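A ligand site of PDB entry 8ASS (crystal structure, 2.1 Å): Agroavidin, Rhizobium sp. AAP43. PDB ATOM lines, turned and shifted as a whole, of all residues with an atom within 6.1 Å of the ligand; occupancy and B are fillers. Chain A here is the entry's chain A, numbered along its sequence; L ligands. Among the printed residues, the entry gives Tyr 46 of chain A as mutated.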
ATOM      1  N   ASN A  26      27.244  -9.946   0.849  1.00  0.00           N
ATOM      2  CA  ASN A  26      28.654  -9.516   1.057  1.00  0.00           C
ATOM      3  C   ASN A  26      28.676  -8.274   1.954  1.00  0.00           C
ATOM      4  O   ASN A  26      27.582  -7.740   2.262  1.00  0.00           O
ATOM      5  CB  ASN A  26      29.451  -9.378  -0.250  1.00  0.00           C
ATOM      6  CG  ASN A  26      28.878  -8.438  -1.286  1.00  0.00           C
ATOM      7  OD1 ASN A  26      28.248  -7.440  -0.946  1.00  0.00           O
ATOM      8  ND2 ASN A  26      29.123  -8.715  -2.559  1.00  0.00           N
ATOM      9  N   LEU A  28      29.372  -5.407   1.182  1.00  0.00           N
ATOM     10  CA  LEU A  28      28.828  -4.265   0.407  1.00  0.00           C
ATOM     11  C   LEU A  28      27.311  -4.321   0.392  1.00  0.00           C
ATOM     12  O   LEU A  28      26.706  -3.351  -0.075  1.00  0.00           O
ATOM     13  CB  LEU A  28      29.325  -4.313  -1.035  1.00  0.00           C
ATOM     14  CG  LEU A  28      30.838  -4.191  -1.232  1.00  0.00           C
ATOM     15  CD1 LEU A  28      31.137  -4.273  -2.728  1.00  0.00           C
ATOM     16  CD2 LEU A  28      31.378  -2.899  -0.619  1.00  0.00           C
ATOM     17  N   SER A  30      25.461  -6.658  -1.142  1.00  0.00           N
ATOM     18  CA  SER A  30      24.960  -7.379  -2.326  1.00  0.00           C
ATOM     19  C   SER A  30      24.463  -8.746  -1.888  1.00  0.00           C
ATOM     20  O   SER A  30      25.029  -9.285  -0.929  1.00  0.00           O
ATOM     21  CB  SER A  30      26.008  -7.510  -3.411  1.00  0.00           C
ATOM     22  OG  SER A  30      26.363  -6.235  -3.918  1.00  0.00           O
ATOM     23  N   TYR A  46      22.403 -12.336  -9.170  1.00  0.00           N
ATOM     24  CA  TYR A  46      23.162 -11.422  -8.282  1.00  0.00           C
ATOM     25  C   TYR A  46      22.339 -10.138  -8.200  1.00  0.00           C
ATOM     26  O   TYR A  46      21.709  -9.797  -9.224  1.00  0.00           O
ATOM     27  CB  TYR A  46      24.576 -11.146  -8.806  1.00  0.00           C
ATOM     28  CG  TYR A  46      25.565 -10.643  -7.777  1.00  0.00           C
ATOM     29  CD1 TYR A  46      25.654  -9.281  -7.487  1.00  0.00           C
ATOM     30  CD2 TYR A  46      26.443 -11.507  -7.136  1.00  0.00           C
ATOM     31  CE1 TYR A  46      26.607  -8.807  -6.592  1.00  0.00           C
ATOM     32  CE2 TYR A  46      27.381 -11.044  -6.230  1.00  0.00           C
ATOM     33  CZ  TYR A  46      27.469  -9.684  -5.975  1.00  0.00           C
ATOM     34  OH  TYR A  46      28.365  -9.202  -5.072  1.00  0.00           O
ATOM     35  N   VAL A  47      22.304  -9.561  -6.998  1.00  0.00           N
ATOM     36  CA  VAL A  47      21.680  -8.249  -6.687  1.00  0.00           C
ATOM     37  C   VAL A  47      22.759  -7.405  -6.012  1.00  0.00           C
ATOM     38  O   VAL A  47      23.148  -7.733  -4.860  1.00  0.00           O
ATOM     39  CB  VAL A  47      20.422  -8.389  -5.791  1.00  0.00           C
ATOM     40  CG1 VAL A  47      19.645  -7.086  -5.807  1.00  0.00           C
ATOM     41  CG2 VAL A  47      19.522  -9.554  -6.192  1.00  0.00           C
ATOM     42  N   ASN A  48      23.214  -6.360  -6.712  1.00  0.00           N
ATOM     43  CA  ASN A  48      24.285  -5.441  -6.273  1.00  0.00           C
ATOM     44  C   ASN A  48      23.643  -4.303  -5.481  1.00  0.00           C
ATOM     45  O   ASN A  48      22.584  -3.824  -5.890  1.00  0.00           O
ATOM     46  CB  ASN A  48      25.099  -4.953  -7.487  1.00  0.00           C
ATOM     47  CG  ASN A  48      26.001  -3.765  -7.206  1.00  0.00           C
ATOM     48  OD1 ASN A  48      26.793  -3.768  -6.265  1.00  0.00           O
ATOM     49  ND2 ASN A  48      25.904  -2.744  -8.042  1.00  0.00           N
ATOM     50  N   ASN A  49      24.268  -3.865  -4.390  1.00  0.00           N
ATOM     51  CA  ASN A  49      23.890  -2.587  -3.755  1.00  0.00           C
ATOM     52  C   ASN A  49      25.138  -1.799  -3.342  1.00  0.00           C
ATOM     53  O   ASN A  49      25.005  -0.907  -2.493  1.00  0.00           O
ATOM     54  CB  ASN A  49      22.934  -2.808  -2.580  1.00  0.00           C
ATOM     55  CG  ASN A  49      22.347  -1.513  -2.070  1.00  0.00           C
ATOM     56  OD1 ASN A  49      22.080  -0.590  -2.838  1.00  0.00           O
ATOM     57  ND2 ASN A  49      22.190  -1.431  -0.760  1.00  0.00           N
ATOM     58  N   ALA A  50      26.287  -2.067  -3.965  1.00  0.00           N
ATOM     59  CA  ALA A  50      27.583  -1.468  -3.581  1.00  0.00           C
ATOM     60  C   ALA A  50      27.503   0.057  -3.672  1.00  0.00           C
ATOM     61  O   ALA A  50      27.184   0.589  -4.695  1.00  0.00           O
ATOM     62  CB  ALA A  50      28.694  -2.005  -4.445  1.00  0.00           C
ATOM     63  N   GLY A  52      28.346   3.469  -4.767  1.00  0.00           N
ATOM     64  CA  GLY A  52      29.067   4.177  -5.847  1.00  0.00           C
ATOM     65  C   GLY A  52      29.088   3.400  -7.159  1.00  0.00           C
ATOM     66  O   GLY A  52      29.865   3.795  -8.060  1.00  0.00           O
ATOM     67  N   THR A  53      28.268   2.351  -7.281  1.00  0.00           N
ATOM     68  CA  THR A  53      28.180   1.522  -8.514  1.00  0.00           C
ATOM     69  C   THR A  53      26.824   1.751  -9.172  1.00  0.00           C
ATOM     70  O   THR A  53      25.934   2.283  -8.514  1.00  0.00           O
ATOM     71  CB  THR A  53      28.438   0.032  -8.251  1.00  0.00           C
ATOM     72  OG1 THR A  53      27.414  -0.508  -7.420  1.00  0.00           O
ATOM     73  CG2 THR A  53      29.795  -0.210  -7.621  1.00  0.00           C
ATOM     74  N   GLY A  54      26.697   1.364 -10.426  1.00  0.00           N
ATOM     75  CA  GLY A  54      25.417   1.325 -11.149  1.00  0.00           C
ATOM     76  C   GLY A  54      24.716   0.014 -10.900  1.00  0.00           C
ATOM     77  O   GLY A  54      25.265  -0.778 -10.131  1.00  0.00           O
ATOM     78  N   CYS A  55      23.548  -0.163 -11.520  1.00  0.00           N
ATOM     79  CA  CYS A  55      22.781  -1.410 -11.670  1.00  0.00           C
ATOM     80  C   CYS A  55      22.406  -1.981 -10.297  1.00  0.00           C
ATOM     81  O   CYS A  55      22.463  -3.211 -10.140  1.00  0.00           O
ATOM     82  CB  CYS A  55      23.571  -2.405 -12.527  1.00  0.00           C
ATOM     83  SG  CYS A  55      23.619  -1.934 -14.276  1.00  0.00           S
ATOM     84  N   TRP A  77      26.409  -7.299 -16.324  1.00  0.00           N
ATOM     85  CA  TRP A  77      25.413  -6.292 -15.862  1.00  0.00           C
ATOM     86  C   TRP A  77      24.531  -5.779 -17.013  1.00  0.00           C
ATOM     87  O   TRP A  77      24.584  -4.584 -17.315  1.00  0.00           O
ATOM     88  CB  TRP A  77      26.160  -5.157 -15.173  1.00  0.00           C
ATOM     89  CG  TRP A  77      27.043  -5.671 -14.080  1.00  0.00           C
ATOM     90  CD1 TRP A  77      28.401  -5.757 -14.100  1.00  0.00           C
ATOM     91  CD2 TRP A  77      26.598  -6.210 -12.837  1.00  0.00           C
ATOM     92  NE1 TRP A  77      28.841  -6.294 -12.923  1.00  0.00           N
ATOM     93  CE2 TRP A  77      27.760  -6.555 -12.119  1.00  0.00           C
ATOM     94  CE3 TRP A  77      25.348  -6.351 -12.219  1.00  0.00           C
ATOM     95  CZ2 TRP A  77      27.701  -7.045 -10.816  1.00  0.00           C
ATOM     96  CZ3 TRP A  77      25.291  -6.854 -10.943  1.00  0.00           C
ATOM     97  CH2 TRP A  77      26.446  -7.216 -10.257  1.00  0.00           C
ATOM     98  N   CYS A  84      24.935  -1.665 -17.364  1.00  0.00           N
ATOM     99  CA  CYS A  84      26.061  -0.768 -16.975  1.00  0.00           C
ATOM    100  C   CYS A  84      27.278  -1.116 -17.837  1.00  0.00           C
ATOM    101  O   CYS A  84      28.371  -0.631 -17.537  1.00  0.00           O
ATOM    102  CB  CYS A  84      26.350  -0.837 -15.467  1.00  0.00           C
ATOM    103  SG  CYS A  84      24.965  -0.359 -14.399  1.00  0.00           S
ATOM    104  N   ARG A  85      27.095  -1.899 -18.916  1.00  0.00           N
ATOM    105  CA  ARG A  85      28.113  -2.175 -19.972  1.00  0.00           C
ATOM    106  C   ARG A  85      29.390  -2.749 -19.332  1.00  0.00           C
ATOM    107  O   ARG A  85      30.500  -2.306 -19.683  1.00  0.00           O
ATOM    108  CB  ARG A  85      28.498  -0.885 -20.705  1.00  0.00           C
ATOM    109  CG  ARG A  85      27.351  -0.183 -21.410  1.00  0.00           C
ATOM    110  CD  ARG A  85      27.615   1.310 -21.477  1.00  0.00           C
ATOM    111  NE  ARG A  85      27.210   1.896 -22.749  1.00  0.00           N
ATOM    112  CZ  ARG A  85      27.104   3.199 -22.988  1.00  0.00           C
ATOM    113  NH1 ARG A  85      26.730   3.612 -24.186  1.00  0.00           N
ATOM    114  NH2 ARG A  85      27.353   4.077 -22.031  1.00  0.00           N
ATOM    115  N   SER A  86      29.230  -3.644 -18.361  1.00  0.00           N
ATOM    116  CA  SER A  86      30.363  -4.181 -17.571  1.00  0.00           C
ATOM    117  C   SER A  86      30.093  -5.633 -17.210  1.00  0.00           C
ATOM    118  O   SER A  86      28.972  -6.125 -17.468  1.00  0.00           O
ATOM    119  CB  SER A  86      30.654  -3.316 -16.350  1.00  0.00           C
ATOM    120  OG  SER A  86      29.503  -2.972 -15.608  1.00  0.00           O
ATOM    121  N   ALA A  87      31.098  -6.308 -16.673  1.00  0.00           N
ATOM    122  CA  ALA A  87      31.026  -7.738 -16.287  1.00  0.00           C
ATOM    123  C   ALA A  87      31.908  -7.964 -15.072  1.00  0.00           C
ATOM    124  O   ALA A  87      32.969  -7.322 -14.980  1.00  0.00           O
ATOM    125  CB  ALA A  87      31.454  -8.597 -17.456  1.00  0.00           C
ATOM    126  N   THR A  88      31.473  -8.840 -14.163  1.00  0.00           N
ATOM    127  CA  THR A  88      32.280  -9.259 -13.005  1.00  0.00           C
ATOM    128  C   THR A  88      32.361 -10.785 -12.973  1.00  0.00           C
ATOM    129  O   THR A  88      31.407 -11.493 -13.350  1.00  0.00           O
ATOM    130  CB  THR A  88      31.760  -8.661 -11.690  1.00  0.00           C
ATOM    131  OG1 THR A  88      31.980  -7.264 -11.778  1.00  0.00           O
ATOM    132  CG2 THR A  88      32.501  -9.164 -10.478  1.00  0.00           C
ATOM    133  N   TRP A  90      34.028 -13.523  -9.993  1.00  0.00           N
ATOM    134  CA  TRP A  90      34.630 -13.778  -8.672  1.00  0.00           C
ATOM    135  C   TRP A  90      35.228 -15.188  -8.701  1.00  0.00           C
ATOM    136  O   TRP A  90      34.584 -16.084  -9.278  1.00  0.00           O
ATOM    137  CB  TRP A  90      33.585 -13.705  -7.535  1.00  0.00           C
ATOM    138  CG  TRP A  90      32.872 -12.410  -7.264  1.00  0.00           C
ATOM    139  CD1 TRP A  90      33.025 -11.636  -6.157  1.00  0.00           C
ATOM    140  CD2 TRP A  90      31.818 -11.802  -8.037  1.00  0.00           C
ATOM    141  NE1 TRP A  90      32.190 -10.551  -6.208  1.00  0.00           N
ATOM    142  CE2 TRP A  90      31.421 -10.649  -7.349  1.00  0.00           C
ATOM    143  CE3 TRP A  90      31.189 -12.110  -9.249  1.00  0.00           C
ATOM    144  CZ2 TRP A  90      30.421  -9.794  -7.821  1.00  0.00           C
ATOM    145  CZ3 TRP A  90      30.197 -11.274  -9.712  1.00  0.00           C
ATOM    146  CH2 TRP A  90      29.814 -10.135  -9.010  1.00  0.00           C
ATOM    147  N   TRP A 108      37.278 -10.357  -6.946  1.00  0.00           N
ATOM    148  CA  TRP A 108      36.453 -10.014  -8.139  1.00  0.00           C
ATOM    149  C   TRP A 108      37.306  -9.092  -9.007  1.00  0.00           C
ATOM    150  O   TRP A 108      38.157  -8.318  -8.426  1.00  0.00           O
ATOM    151  CB  TRP A 108      35.130  -9.347  -7.737  1.00  0.00           C
ATOM    152  CG  TRP A 108      35.299  -8.134  -6.870  1.00  0.00           C
ATOM    153  CD1 TRP A 108      35.304  -8.106  -5.508  1.00  0.00           C
ATOM    154  CD2 TRP A 108      35.504  -6.782  -7.297  1.00  0.00           C
ATOM    155  NE1 TRP A 108      35.498  -6.836  -5.055  1.00  0.00           N
ATOM    156  CE2 TRP A 108      35.593  -5.990  -6.123  1.00  0.00           C
ATOM    157  CE3 TRP A 108      35.626  -6.144  -8.541  1.00  0.00           C
ATOM    158  CZ2 TRP A 108      35.817  -4.613  -6.157  1.00  0.00           C
ATOM    159  CZ3 TRP A 108      35.819  -4.777  -8.583  1.00  0.00           C
ATOM    160  CH2 TRP A 108      35.921  -4.026  -7.404  1.00  0.00           C
ATOM    161  N   LEU A 110      36.378  -6.427 -12.246  1.00  0.00           N
ATOM    162  CA  LEU A 110      35.253  -5.757 -12.928  1.00  0.00           C
ATOM    163  C   LEU A 110      35.787  -5.142 -14.228  1.00  0.00           C
ATOM    164  O   LEU A 110      36.673  -4.280 -14.103  1.00  0.00           O
ATOM    165  CB  LEU A 110      34.660  -4.702 -11.986  1.00  0.00           C
ATOM    166  CG  LEU A 110      33.652  -3.721 -12.571  1.00  0.00           C
ATOM    167  CD1 LEU A 110      32.611  -4.407 -13.431  1.00  0.00           C
ATOM    168  CD2 LEU A 110      32.977  -2.944 -11.439  1.00  0.00           C
ATOM    169  N   PHE A 112      34.982  -3.039 -17.727  1.00  0.00           N
ATOM    170  CA  PHE A 112      34.148  -2.032 -18.450  1.00  0.00           C
ATOM    171  C   PHE A 112      35.029  -1.343 -19.490  1.00  0.00           C
ATOM    172  O   PHE A 112      36.256  -1.257 -19.259  1.00  0.00           O
ATOM    173  CB  PHE A 112      33.564  -0.996 -17.499  1.00  0.00           C
ATOM    174  CG  PHE A 112      34.562  -0.207 -16.685  1.00  0.00           C
ATOM    175  CD1 PHE A 112      35.075  -0.716 -15.496  1.00  0.00           C
ATOM    176  CD2 PHE A 112      34.998   1.042 -17.100  1.00  0.00           C
ATOM    177  CE1 PHE A 112      35.985   0.020 -14.745  1.00  0.00           C
ATOM    178  CE2 PHE A 112      35.914   1.770 -16.349  1.00  0.00           C
ATOM    179  CZ  PHE A 112      36.397   1.264 -15.163  1.00  0.00           C
ATOM    180  N   ASN A 125      35.729  -9.628  -1.873  1.00  0.00           N
ATOM    181  CA  ASN A 125      34.357  -9.761  -1.314  1.00  0.00           C
ATOM    182  C   ASN A 125      34.298 -11.007  -0.436  1.00  0.00           C
ATOM    183  O   ASN A 125      34.849 -12.064  -0.825  1.00  0.00           O
ATOM    184  CB  ASN A 125      33.241  -9.862  -2.362  1.00  0.00           C
ATOM    185  CG  ASN A 125      32.782  -8.541  -2.962  1.00  0.00           C
ATOM    186  OD1 ASN A 125      32.149  -8.550  -4.003  1.00  0.00           O
ATOM    187  ND2 ASN A 125      33.087  -7.409  -2.347  1.00  0.00           N
ATOM    188  N   PHE A 127      31.390 -13.304   1.015  1.00  0.00           N
ATOM    189  CA  PHE A 127      29.962 -13.689   1.072  1.00  0.00           C
ATOM    190  C   PHE A 127      29.728 -14.520   2.345  1.00  0.00           C
ATOM    191  O   PHE A 127      30.589 -15.343   2.699  1.00  0.00           O
ATOM    192  CB  PHE A 127      29.535 -14.433  -0.187  1.00  0.00           C
ATOM    193  CG  PHE A 127      29.671 -13.587  -1.423  1.00  0.00           C
ATOM    194  CD1 PHE A 127      30.918 -13.359  -1.990  1.00  0.00           C
ATOM    195  CD2 PHE A 127      28.552 -13.009  -2.004  1.00  0.00           C
ATOM    196  CE1 PHE A 127      31.051 -12.563  -3.115  1.00  0.00           C
ATOM    197  CE2 PHE A 127      28.683 -12.225  -3.134  1.00  0.00           C
ATOM    198  CZ  PHE A 127      29.940 -11.990  -3.682  1.00  0.00           C
HETATM  199  C1  LIG L   1      29.023  -1.356 -12.550  1.00  0.00           C
HETATM  200  O1  LIG L   1      29.815  -1.411 -13.528  1.00  0.00           O
HETATM  201  O2  LIG L   1      29.037  -0.430 -11.696  1.00  0.00           O
HETATM  202  C2  LIG L   1      27.979  -2.461 -12.382  1.00  0.00           C
HETATM  203  C3  LIG L   1      27.839  -2.971 -10.974  1.00  0.00           C
HETATM  204  C4  LIG L   1      29.116  -3.595 -10.399  1.00  0.00           C
HETATM  205  C5  LIG L   1      29.042  -3.968  -8.922  1.00  0.00           C
HETATM  206  C6  LIG L   1      30.379  -4.286  -8.269  1.00  0.00           C
HETATM  207  S1  LIG L   1      30.879  -5.944  -8.844  1.00  0.00           S
HETATM  208  C7  LIG L   1      32.200  -5.786  -7.602  1.00  0.00           C
HETATM  209  C8  LIG L   1      31.564  -5.261  -6.313  1.00  0.00           C
HETATM  210  N1  LIG L   1      30.903  -6.268  -5.517  1.00  0.00           N
HETATM  211  C9  LIG L   1      29.571  -6.075  -5.424  1.00  0.00           C
HETATM  212  O3  LIG L   1      28.759  -6.788  -4.815  1.00  0.00           O
HETATM  213  N2  LIG L   1      29.261  -4.971  -6.140  1.00  0.00           N
HETATM  214  C10 LIG L   1      30.417  -4.328  -6.727  1.00  0.00           C
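The side-chain hydroxyl of Tyr 46 lies within hydrogen-bond range of an oxygen (O3) of the ligand, at 2.5 Å.
The side-chain hydroxyl (OG) of Ser 30 sits at hydrogen-bond distance from an oxygen (O3) of the ligand (2.6 Å).
An oxygen (O1) of the ligand is in hydrogen-bond range of the side-chain hydroxyl (OG) of Ser 86, 2.6 Å away.
OD1 of Asn 48 is in hydrogen-bond range of N2 of the ligand, 2.7 Å away.
O3 of the ligand lies within hydrogen-bond range of ND2 of Asn 26 (3.0 Å).
The side-chain amide oxygen of Asn 125 lies within hydrogen-bond range of a nitrogen (N1) of the ligand, 3.0 Å away.
The backbone NH (N) of Gly 54 sits at hydrogen-bond distance from an oxygen (O2) of the ligand.
The side-chain hydroxyl of Thr 88 lies close to a sulfur (S1) of the ligand (3.4 Å).
Merely in contact with the ligand: Leu 28, Ala 50, Trp 108, Thr 53, Trp 77 and Cys 84.
Hydrophobic or aromatic side chains within 4 Å of the ligand: Leu 28, Tyr 46, Ala 50, Trp 77 and Trp 108.
Of the 24 residues printed, 14 come within 4 Å of the ligand.
OG of Ser 30 lies close to OD1 of Asn 48 (3.4 Å).
The backbone NH of Asn 49 sits at hydrogen-bond distance from the side-chain hydroxyl of Ser 30.
N of Trp 77 sits at hydrogen-bond distance from O of Ser 86 (3.0 Å).
OG of Ser 86 sits at hydrogen-bond distance from O of Cys 84 (3.2 Å).
The side-chain amide nitrogen (ND2) of Asn 48 is in hydrogen-bond range of the side-chain hydroxyl (OG1) of Thr 53 (2.8 Å).
The side-chain amide nitrogen (ND2) of Asn 26 sits at hydrogen-bond distance from the side-chain amide oxygen (OD1) of Asn 125 (3.4 Å).
The side-chain amide oxygen (OD1) of Asn 125 is in hydrogen-bond range of the indole nitrogen (NE1) of Trp 90, at 3.0 Å.
OG1 of Thr 53 lies within hydrogen-bond range of O of Ala 50 (2.9 Å).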
